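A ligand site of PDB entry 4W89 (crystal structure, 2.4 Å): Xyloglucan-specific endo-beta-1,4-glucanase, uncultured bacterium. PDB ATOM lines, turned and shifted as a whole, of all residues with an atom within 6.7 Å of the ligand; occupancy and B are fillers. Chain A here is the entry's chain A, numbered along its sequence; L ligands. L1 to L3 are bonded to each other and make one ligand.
The backbone carbonyl oxygen (O) of Glu 149 is in hydrogen-bond range of the guanidinium group (NH1) of Arg 151, at 2.9 Å. A ring nitrogen (ND1) of His 200 sits at hydrogen-bond distance from the backbone NH of Glu 149 (3.1 Å). The side-chain carboxylate (OE2) of Glu 149 is in hydrogen-bond range of a ring nitrogen (ND1) of His 223, at 2.8 Å.
Trp 159 touches the ligand. Tyr 228 touches the ligand. CZ of Phe 229 touches O5 of LIG L1, at 3.8 Å. Hydrophobic or aromatic side chains within 4 Å of the ligand: Trp 159, Tyr 228, Phe 229 and Tyr 232. Five residues have an atom within 4 Å of the ligand: Glu 149, Trp 159, Tyr 228, Phe 229 and Tyr 232.
The side-chain carboxylate (OE2) of Glu 149 is in hydrogen-bond range of an oxygen (O3) of LG3 L3 (2.7 Å). OH of Tyr 232 is in hydrogen-bond range of O2 of LG3 L3 (2.7 Å).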
ATOM      1  N   ASN A 148      -1.677  16.425  -6.188  1.00  0.00           N
ATOM      2  CA  ASN A 148      -2.299  15.873  -4.987  1.00  0.00           C
ATOM      3  C   ASN A 148      -3.781  16.224  -4.887  1.00  0.00           C
ATOM      4  O   ASN A 148      -4.159  17.392  -4.829  1.00  0.00           O
ATOM      5  CB  ASN A 148      -1.596  16.323  -3.723  1.00  0.00           C
ATOM      6  CG  ASN A 148      -2.140  15.615  -2.488  1.00  0.00           C
ATOM      7  OD1 ASN A 148      -1.830  14.453  -2.230  1.00  0.00           O
ATOM      8  ND2 ASN A 148      -2.983  16.313  -1.738  1.00  0.00           N
ATOM      9  N   GLU A 149      -4.593  15.175  -4.829  1.00  0.00           N
ATOM     10  CA  GLU A 149      -6.044  15.264  -4.739  1.00  0.00           C
ATOM     11  C   GLU A 149      -6.628  16.386  -5.596  1.00  0.00           C
ATOM     12  O   GLU A 149      -7.357  17.241  -5.082  1.00  0.00           O
ATOM     13  CB  GLU A 149      -6.447  15.413  -3.277  1.00  0.00           C
ATOM     14  CG  GLU A 149      -5.975  14.261  -2.417  1.00  0.00           C
ATOM     15  CD  GLU A 149      -6.274  14.449  -0.946  1.00  0.00           C
ATOM     16  OE1 GLU A 149      -6.661  15.574  -0.540  1.00  0.00           O
ATOM     17  OE2 GLU A 149      -6.124  13.466  -0.192  1.00  0.00           O
ATOM     18  N   ARG A 151      -8.943  18.562  -7.586  1.00  0.00           N
ATOM     19  CA  ARG A 151     -10.383  18.617  -7.421  1.00  0.00           C
ATOM     20  C   ARG A 151     -10.890  20.054  -7.412  1.00  0.00           C
ATOM     21  O   ARG A 151     -10.107  21.003  -7.383  1.00  0.00           O
ATOM     22  CB  ARG A 151     -10.786  17.946  -6.111  1.00  0.00           C
ATOM     23  CG  ARG A 151     -10.315  18.700  -4.873  1.00  0.00           C
ATOM     24  CD  ARG A 151     -10.329  17.839  -3.636  1.00  0.00           C
ATOM     25  NE  ARG A 151     -10.101  18.649  -2.438  1.00  0.00           N
ATOM     26  CZ  ARG A 151      -8.911  19.080  -2.012  1.00  0.00           C
ATOM     27  NH1 ARG A 151      -7.796  18.791  -2.680  1.00  0.00           N
ATOM     28  NH2 ARG A 151      -8.823  19.799  -0.911  1.00  0.00           N
ATOM     29  N   TRP A 159     -15.174  15.105  -2.778  1.00  0.00           N
ATOM     30  CA  TRP A 159     -14.567  13.967  -2.107  1.00  0.00           C
ATOM     31  C   TRP A 159     -15.152  12.627  -2.547  1.00  0.00           C
ATOM     32  O   TRP A 159     -15.007  11.625  -1.839  1.00  0.00           O
ATOM     33  CB  TRP A 159     -14.737  14.117  -0.598  1.00  0.00           C
ATOM     34  CG  TRP A 159     -14.060  15.337  -0.055  1.00  0.00           C
ATOM     35  CD1 TRP A 159     -14.656  16.380   0.582  1.00  0.00           C
ATOM     36  CD2 TRP A 159     -12.667  15.632  -0.109  1.00  0.00           C
ATOM     37  NE1 TRP A 159     -13.721  17.309   0.944  1.00  0.00           N
ATOM     38  CE2 TRP A 159     -12.490  16.886   0.530  1.00  0.00           C
ATOM     39  CE3 TRP A 159     -11.546  14.986  -0.636  1.00  0.00           C
ATOM     40  CZ2 TRP A 159     -11.235  17.479   0.662  1.00  0.00           C
ATOM     41  CZ3 TRP A 159     -10.304  15.577  -0.511  1.00  0.00           C
ATOM     42  CH2 TRP A 159     -10.153  16.816   0.133  1.00  0.00           C
ATOM     43  N   SER A 160     -15.809  12.581  -3.702  1.00  0.00           N
ATOM     44  CA  SER A 160     -16.304  11.320  -4.231  1.00  0.00           C
ATOM     45  C   SER A 160     -16.126  11.231  -5.734  1.00  0.00           C
ATOM     46  O   SER A 160     -17.006  10.736  -6.448  1.00  0.00           O
ATOM     47  CB  SER A 160     -17.765  11.104  -3.831  1.00  0.00           C
ATOM     48  OG  SER A 160     -18.595  12.068  -4.435  1.00  0.00           O
ATOM     49  N   GLY A 199      -9.239  13.790  -7.124  1.00  0.00           N
ATOM     50  CA  GLY A 199      -9.184  13.723  -5.664  1.00  0.00           C
ATOM     51  C   GLY A 199      -8.470  12.525  -5.060  1.00  0.00           C
ATOM     52  O   GLY A 199      -8.542  12.311  -3.857  1.00  0.00           O
ATOM     53  N   HIS A 200      -7.740  11.777  -5.889  1.00  0.00           N
ATOM     54  CA  HIS A 200      -7.158  10.490  -5.485  1.00  0.00           C
ATOM     55  C   HIS A 200      -8.230   9.457  -5.062  1.00  0.00           C
ATOM     56  O   HIS A 200      -7.916   8.493  -4.359  1.00  0.00           O
ATOM     57  CB  HIS A 200      -6.118  10.676  -4.375  1.00  0.00           C
ATOM     58  CG  HIS A 200      -4.732  10.937  -4.867  1.00  0.00           C
ATOM     59  ND1 HIS A 200      -4.376  12.119  -5.472  1.00  0.00           N
ATOM     60  CD2 HIS A 200      -3.607  10.192  -4.810  1.00  0.00           C
ATOM     61  CE1 HIS A 200      -3.087  12.082  -5.778  1.00  0.00           C
ATOM     62  NE2 HIS A 200      -2.596  10.921  -5.392  1.00  0.00           N
ATOM     63  N   ASN A 201      -9.464   9.662  -5.519  1.00  0.00           N
ATOM     64  CA  ASN A 201     -10.577   8.775  -5.163  1.00  0.00           C
ATOM     65  C   ASN A 201     -10.460   7.436  -5.880  1.00  0.00           C
ATOM     66  O   ASN A 201      -9.985   7.378  -7.016  1.00  0.00           O
ATOM     67  CB  ASN A 201     -11.907   9.459  -5.529  1.00  0.00           C
ATOM     68  CG  ASN A 201     -13.109   8.612  -5.154  1.00  0.00           C
ATOM     69  OD1 ASN A 201     -13.685   7.918  -5.988  1.00  0.00           O
ATOM     70  ND2 ASN A 201     -13.478   8.658  -3.885  1.00  0.00           N
ATOM     71  N   HIS A 223      -5.545   7.601  -2.726  1.00  0.00           N
ATOM     72  CA  HIS A 223      -5.566   7.799  -1.276  1.00  0.00           C
ATOM     73  C   HIS A 223      -6.753   7.051  -0.708  1.00  0.00           C
ATOM     74  O   HIS A 223      -7.875   7.201  -1.168  1.00  0.00           O
ATOM     75  CB  HIS A 223      -5.665   9.275  -0.912  1.00  0.00           C
ATOM     76  CG  HIS A 223      -4.443  10.053  -1.270  1.00  0.00           C
ATOM     77  ND1 HIS A 223      -4.373  11.418  -1.106  1.00  0.00           N
ATOM     78  CD2 HIS A 223      -3.256   9.668  -1.774  1.00  0.00           C
ATOM     79  CE1 HIS A 223      -3.186  11.842  -1.499  1.00  0.00           C
ATOM     80  NE2 HIS A 223      -2.484  10.796  -1.903  1.00  0.00           N
ATOM     81  N   THR A 224      -6.479   6.225   0.294  1.00  0.00           N
ATOM     82  CA  THR A 224      -7.484   5.373   0.888  1.00  0.00           C
ATOM     83  C   THR A 224      -7.286   5.368   2.387  1.00  0.00           C
ATOM     84  O   THR A 224      -6.470   4.619   2.920  1.00  0.00           O
ATOM     85  CB  THR A 224      -7.367   3.931   0.367  1.00  0.00           C
ATOM     86  OG1 THR A 224      -6.004   3.502   0.510  1.00  0.00           O
ATOM     87  CG2 THR A 224      -7.749   3.851  -1.106  1.00  0.00           C
ATOM     88  N   TYR A 225      -8.017   6.244   3.065  1.00  0.00           N
ATOM     89  CA  TYR A 225      -8.050   6.226   4.514  1.00  0.00           C
ATOM     90  C   TYR A 225      -9.258   5.392   4.915  1.00  0.00           C
ATOM     91  O   TYR A 225     -10.143   5.849   5.651  1.00  0.00           O
ATOM     92  CB  TYR A 225      -8.159   7.648   5.054  1.00  0.00           C
ATOM     93  CG  TYR A 225      -6.947   8.526   4.816  1.00  0.00           C
ATOM     94  CD1 TYR A 225      -6.715   9.125   3.580  1.00  0.00           C
ATOM     95  CD2 TYR A 225      -6.050   8.789   5.849  1.00  0.00           C
ATOM     96  CE1 TYR A 225      -5.625   9.953   3.380  1.00  0.00           C
ATOM     97  CE2 TYR A 225      -4.964   9.614   5.658  1.00  0.00           C
ATOM     98  CZ  TYR A 225      -4.750  10.191   4.428  1.00  0.00           C
ATOM     99  OH  TYR A 225      -3.656  11.001   4.269  1.00  0.00           O
ATOM    100  N   TYR A 228     -13.252   5.541   6.252  1.00  0.00           N
ATOM    101  CA  TYR A 228     -13.196   6.922   6.691  1.00  0.00           C
ATOM    102  C   TYR A 228     -13.556   7.115   8.169  1.00  0.00           C
ATOM    103  O   TYR A 228     -12.854   7.816   8.904  1.00  0.00           O
ATOM    104  CB  TYR A 228     -14.118   7.777   5.802  1.00  0.00           C
ATOM    105  CG  TYR A 228     -14.273   9.204   6.262  1.00  0.00           C
ATOM    106  CD1 TYR A 228     -13.203  10.091   6.207  1.00  0.00           C
ATOM    107  CD2 TYR A 228     -15.488   9.680   6.741  1.00  0.00           C
ATOM    108  CE1 TYR A 228     -13.339  11.415   6.621  1.00  0.00           C
ATOM    109  CE2 TYR A 228     -15.633  10.993   7.158  1.00  0.00           C
ATOM    110  CZ  TYR A 228     -14.560  11.850   7.104  1.00  0.00           C
ATOM    111  OH  TYR A 228     -14.701  13.150   7.517  1.00  0.00           O
ATOM    112  N   PHE A 229     -14.625   6.458   8.609  1.00  0.00           N
ATOM    113  CA  PHE A 229     -15.155   6.617   9.975  1.00  0.00           C
ATOM    114  C   PHE A 229     -14.293   5.982  11.068  1.00  0.00           C
ATOM    115  O   PHE A 229     -14.473   6.286  12.242  1.00  0.00           O
ATOM    116  CB  PHE A 229     -16.592   6.109  10.073  1.00  0.00           C
ATOM    117  CG  PHE A 229     -17.607   7.047   9.471  1.00  0.00           C
ATOM    118  CD1 PHE A 229     -17.769   8.327   9.984  1.00  0.00           C
ATOM    119  CD2 PHE A 229     -18.388   6.659   8.396  1.00  0.00           C
ATOM    120  CE1 PHE A 229     -18.684   9.209   9.433  1.00  0.00           C
ATOM    121  CE2 PHE A 229     -19.313   7.525   7.834  1.00  0.00           C
ATOM    122  CZ  PHE A 229     -19.467   8.803   8.363  1.00  0.00           C
ATOM    123  N   TYR A 232     -10.795   8.887  10.423  1.00  0.00           N
ATOM    124  CA  TYR A 232     -11.066  10.294  10.743  1.00  0.00           C
ATOM    125  C   TYR A 232     -12.051  10.437  11.895  1.00  0.00           C
ATOM    126  O   TYR A 232     -12.743   9.488  12.260  1.00  0.00           O
ATOM    127  CB  TYR A 232     -11.632  11.017   9.525  1.00  0.00           C
ATOM    128  CG  TYR A 232     -10.586  11.462   8.543  1.00  0.00           C
ATOM    129  CD1 TYR A 232     -10.040  10.569   7.632  1.00  0.00           C
ATOM    130  CD2 TYR A 232     -10.142  12.786   8.521  1.00  0.00           C
ATOM    131  CE1 TYR A 232      -9.073  10.978   6.726  1.00  0.00           C
ATOM    132  CE2 TYR A 232      -9.175  13.200   7.629  1.00  0.00           C
ATOM    133  CZ  TYR A 232      -8.650  12.298   6.728  1.00  0.00           C
ATOM    134  OH  TYR A 232      -7.704  12.700   5.832  1.00  0.00           O
ATOM    135  N   ALA A 234     -15.433  12.394  13.127  1.00  0.00           N
ATOM    136  CA  ALA A 234     -16.635  12.965  12.504  1.00  0.00           C
ATOM    137  C   ALA A 234     -17.890  12.385  13.167  1.00  0.00           C
ATOM    138  O   ALA A 234     -17.804  11.420  13.932  1.00  0.00           O
ATOM    139  CB  ALA A 234     -16.645  12.651  11.014  1.00  0.00           C
ATOM    140  N   ASP A 235     -19.046  12.965  12.870  1.00  0.00           N
ATOM    141  CA  ASP A 235     -20.308  12.410  13.337  1.00  0.00           C
ATOM    142  C   ASP A 235     -20.547  11.065  12.665  1.00  0.00           C
ATOM    143  O   ASP A 235     -20.748  10.986  11.452  1.00  0.00           O
ATOM    144  CB  ASP A 235     -21.472  13.367  13.062  1.00  0.00           C
ATOM    145  N   GLU A 271      -1.095   8.049   0.120  1.00  0.00           N
ATOM    146  CA  GLU A 271      -1.540   8.433   1.467  1.00  0.00           C
ATOM    147  C   GLU A 271      -2.527   7.438   2.070  1.00  0.00           C
ATOM    148  O   GLU A 271      -3.466   6.976   1.399  1.00  0.00           O
ATOM    149  CB  GLU A 271      -2.184   9.825   1.483  1.00  0.00           C
ATOM    150  CG  GLU A 271      -1.222  11.001   1.411  1.00  0.00           C
ATOM    151  CD  GLU A 271      -1.930  12.344   1.434  1.00  0.00           C
ATOM    152  OE1 GLU A 271      -2.963  12.476   2.114  1.00  0.00           O
ATOM    153  OE2 GLU A 271      -1.440  13.289   0.774  1.00  0.00           O
ATOM    154  N   GLN A 275      -6.164   8.336  12.451  1.00  0.00           N
ATOM    155  CA  GLN A 275      -5.953   9.309  13.517  1.00  0.00           C
ATOM    156  C   GLN A 275      -5.961   8.598  14.867  1.00  0.00           C
ATOM    157  O   GLN A 275      -6.743   7.662  15.084  1.00  0.00           O
ATOM    158  CB  GLN A 275      -7.022  10.401  13.490  1.00  0.00           C
ATOM    159  CG  GLN A 275      -6.954  11.304  12.263  1.00  0.00           C
ATOM    160  CD  GLN A 275      -8.060  12.332  12.239  1.00  0.00           C
ATOM    161  OE1 GLN A 275      -8.573  12.750  13.279  1.00  0.00           O
ATOM    162  NE2 GLN A 275      -8.420  12.782  11.047  1.00  0.00           N
ATOM    163  N   GLU A 314      -5.947  16.852  13.542  1.00  0.00           N
ATOM    164  CA  GLU A 314      -6.060  15.473  13.074  1.00  0.00           C
ATOM    165  C   GLU A 314      -4.811  14.713  13.499  1.00  0.00           C
ATOM    166  O   GLU A 314      -3.714  15.001  13.027  1.00  0.00           O
ATOM    167  CB  GLU A 314      -6.211  15.434  11.556  1.00  0.00           C
ATOM    168  CG  GLU A 314      -7.445  16.152  11.026  1.00  0.00           C
ATOM    169  CD  GLU A 314      -7.525  16.139   9.507  1.00  0.00           C
ATOM    170  OE1 GLU A 314      -6.493  15.927   8.842  1.00  0.00           O
ATOM    171  OE2 GLU A 314      -8.640  16.348   8.980  1.00  0.00           O
ATOM    172  N   PHE A 316      -2.640  12.324  13.087  1.00  0.00           N
ATOM    173  CA  PHE A 316      -1.913  11.384  12.237  1.00  0.00           C
ATOM    174  C   PHE A 316      -0.421  11.279  12.604  1.00  0.00           C
ATOM    175  O   PHE A 316       0.338  10.534  11.971  1.00  0.00           O
ATOM    176  CB  PHE A 316      -2.043  11.799  10.764  1.00  0.00           C
ATOM    177  CG  PHE A 316      -3.393  11.516  10.162  1.00  0.00           C
ATOM    178  CD1 PHE A 316      -3.825  10.204   9.968  1.00  0.00           C
ATOM    179  CD2 PHE A 316      -4.210  12.559   9.741  1.00  0.00           C
ATOM    180  CE1 PHE A 316      -5.059   9.947   9.401  1.00  0.00           C
ATOM    181  CE2 PHE A 316      -5.440  12.305   9.165  1.00  0.00           C
ATOM    182  CZ  PHE A 316      -5.863  10.991   8.987  1.00  0.00           C
HETATM  183  C1  LIG L   1     -20.538  12.109   5.634  1.00  0.00           C
HETATM  184  C2  LIG L   1     -19.442  13.180   5.515  1.00  0.00           C
HETATM  185  C3  LIG L   1     -18.736  13.089   4.171  1.00  0.00           C
HETATM  186  C4  LIG L   1     -18.138  11.681   4.065  1.00  0.00           C
HETATM  187  C5  LIG L   1     -19.299  10.693   3.995  1.00  0.00           C
HETATM  188  C6  LIG L   1     -18.830   9.234   3.897  1.00  0.00           C
HETATM  189  O1  LIG L   1     -21.715  12.543   4.930  1.00  0.00           O
HETATM  190  O2  LIG L   1     -19.996  14.493   5.675  1.00  0.00           O
HETATM  191  O3  LIG L   1     -17.764  14.142   4.088  1.00  0.00           O
HETATM  192  O4  LIG L   1     -17.233  11.559   2.953  1.00  0.00           O
HETATM  193  O5  LIG L   1     -20.135  10.802   5.160  1.00  0.00           O
HETATM  194  O6  LIG L   1     -19.442   8.591   2.778  1.00  0.00           O
HETATM  195  C1  LG2 L   2     -14.831  11.402   2.336  1.00  0.00           C
HETATM  196  C2  LG2 L   2     -13.439  11.866   2.771  1.00  0.00           C
HETATM  197  C3  LG2 L   2     -13.398  13.361   3.142  1.00  0.00           C
HETATM  198  C4  LG2 L   2     -14.617  13.824   3.926  1.00  0.00           C
HETATM  199  C5  LG2 L   2     -14.699  15.340   4.089  1.00  0.00           C
HETATM  200  C6  LG2 L   2     -15.891  11.936   3.302  1.00  0.00           C
HETATM  201  O1  LG2 L   2     -14.864   9.970   2.307  1.00  0.00           O
HETATM  202  O2  LG2 L   2     -12.488  11.606   1.732  1.00  0.00           O
HETATM  203  O3  LG2 L   2     -12.266  13.598   3.973  1.00  0.00           O
HETATM  204  O4  LG2 L   2     -15.794  13.359   3.289  1.00  0.00           O
HETATM  205  O5  LG2 L   2     -13.408  15.898   4.368  1.00  0.00           O
HETATM  206  C1  LG3 L   3     -10.195  14.768   4.271  1.00  0.00           C
HETATM  207  C2  LG3 L   3      -8.785  15.019   3.752  1.00  0.00           C
HETATM  208  C3  LG3 L   3      -8.204  13.873   2.908  1.00  0.00           C
HETATM  209  C4  LG3 L   3      -9.247  13.156   2.030  1.00  0.00           C
HETATM  210  C5  LG3 L   3      -8.718  11.864   1.410  1.00  0.00           C
HETATM  211  C6  LG3 L   3     -11.078  14.002   3.285  1.00  0.00           C
HETATM  212  O1  LG3 L   3     -10.796  16.023   4.587  1.00  0.00           O
HETATM  213  O2  LG3 L   3      -7.914  15.252   4.867  1.00  0.00           O
HETATM  214  O3  LG3 L   3      -7.150  14.444   2.127  1.00  0.00           O
HETATM  215  O4  LG3 L   3     -10.402  12.835   2.805  1.00  0.00           O
HETATM  216  O5  LG3 L   3      -9.662  11.328   0.466  1.00  0.00           O
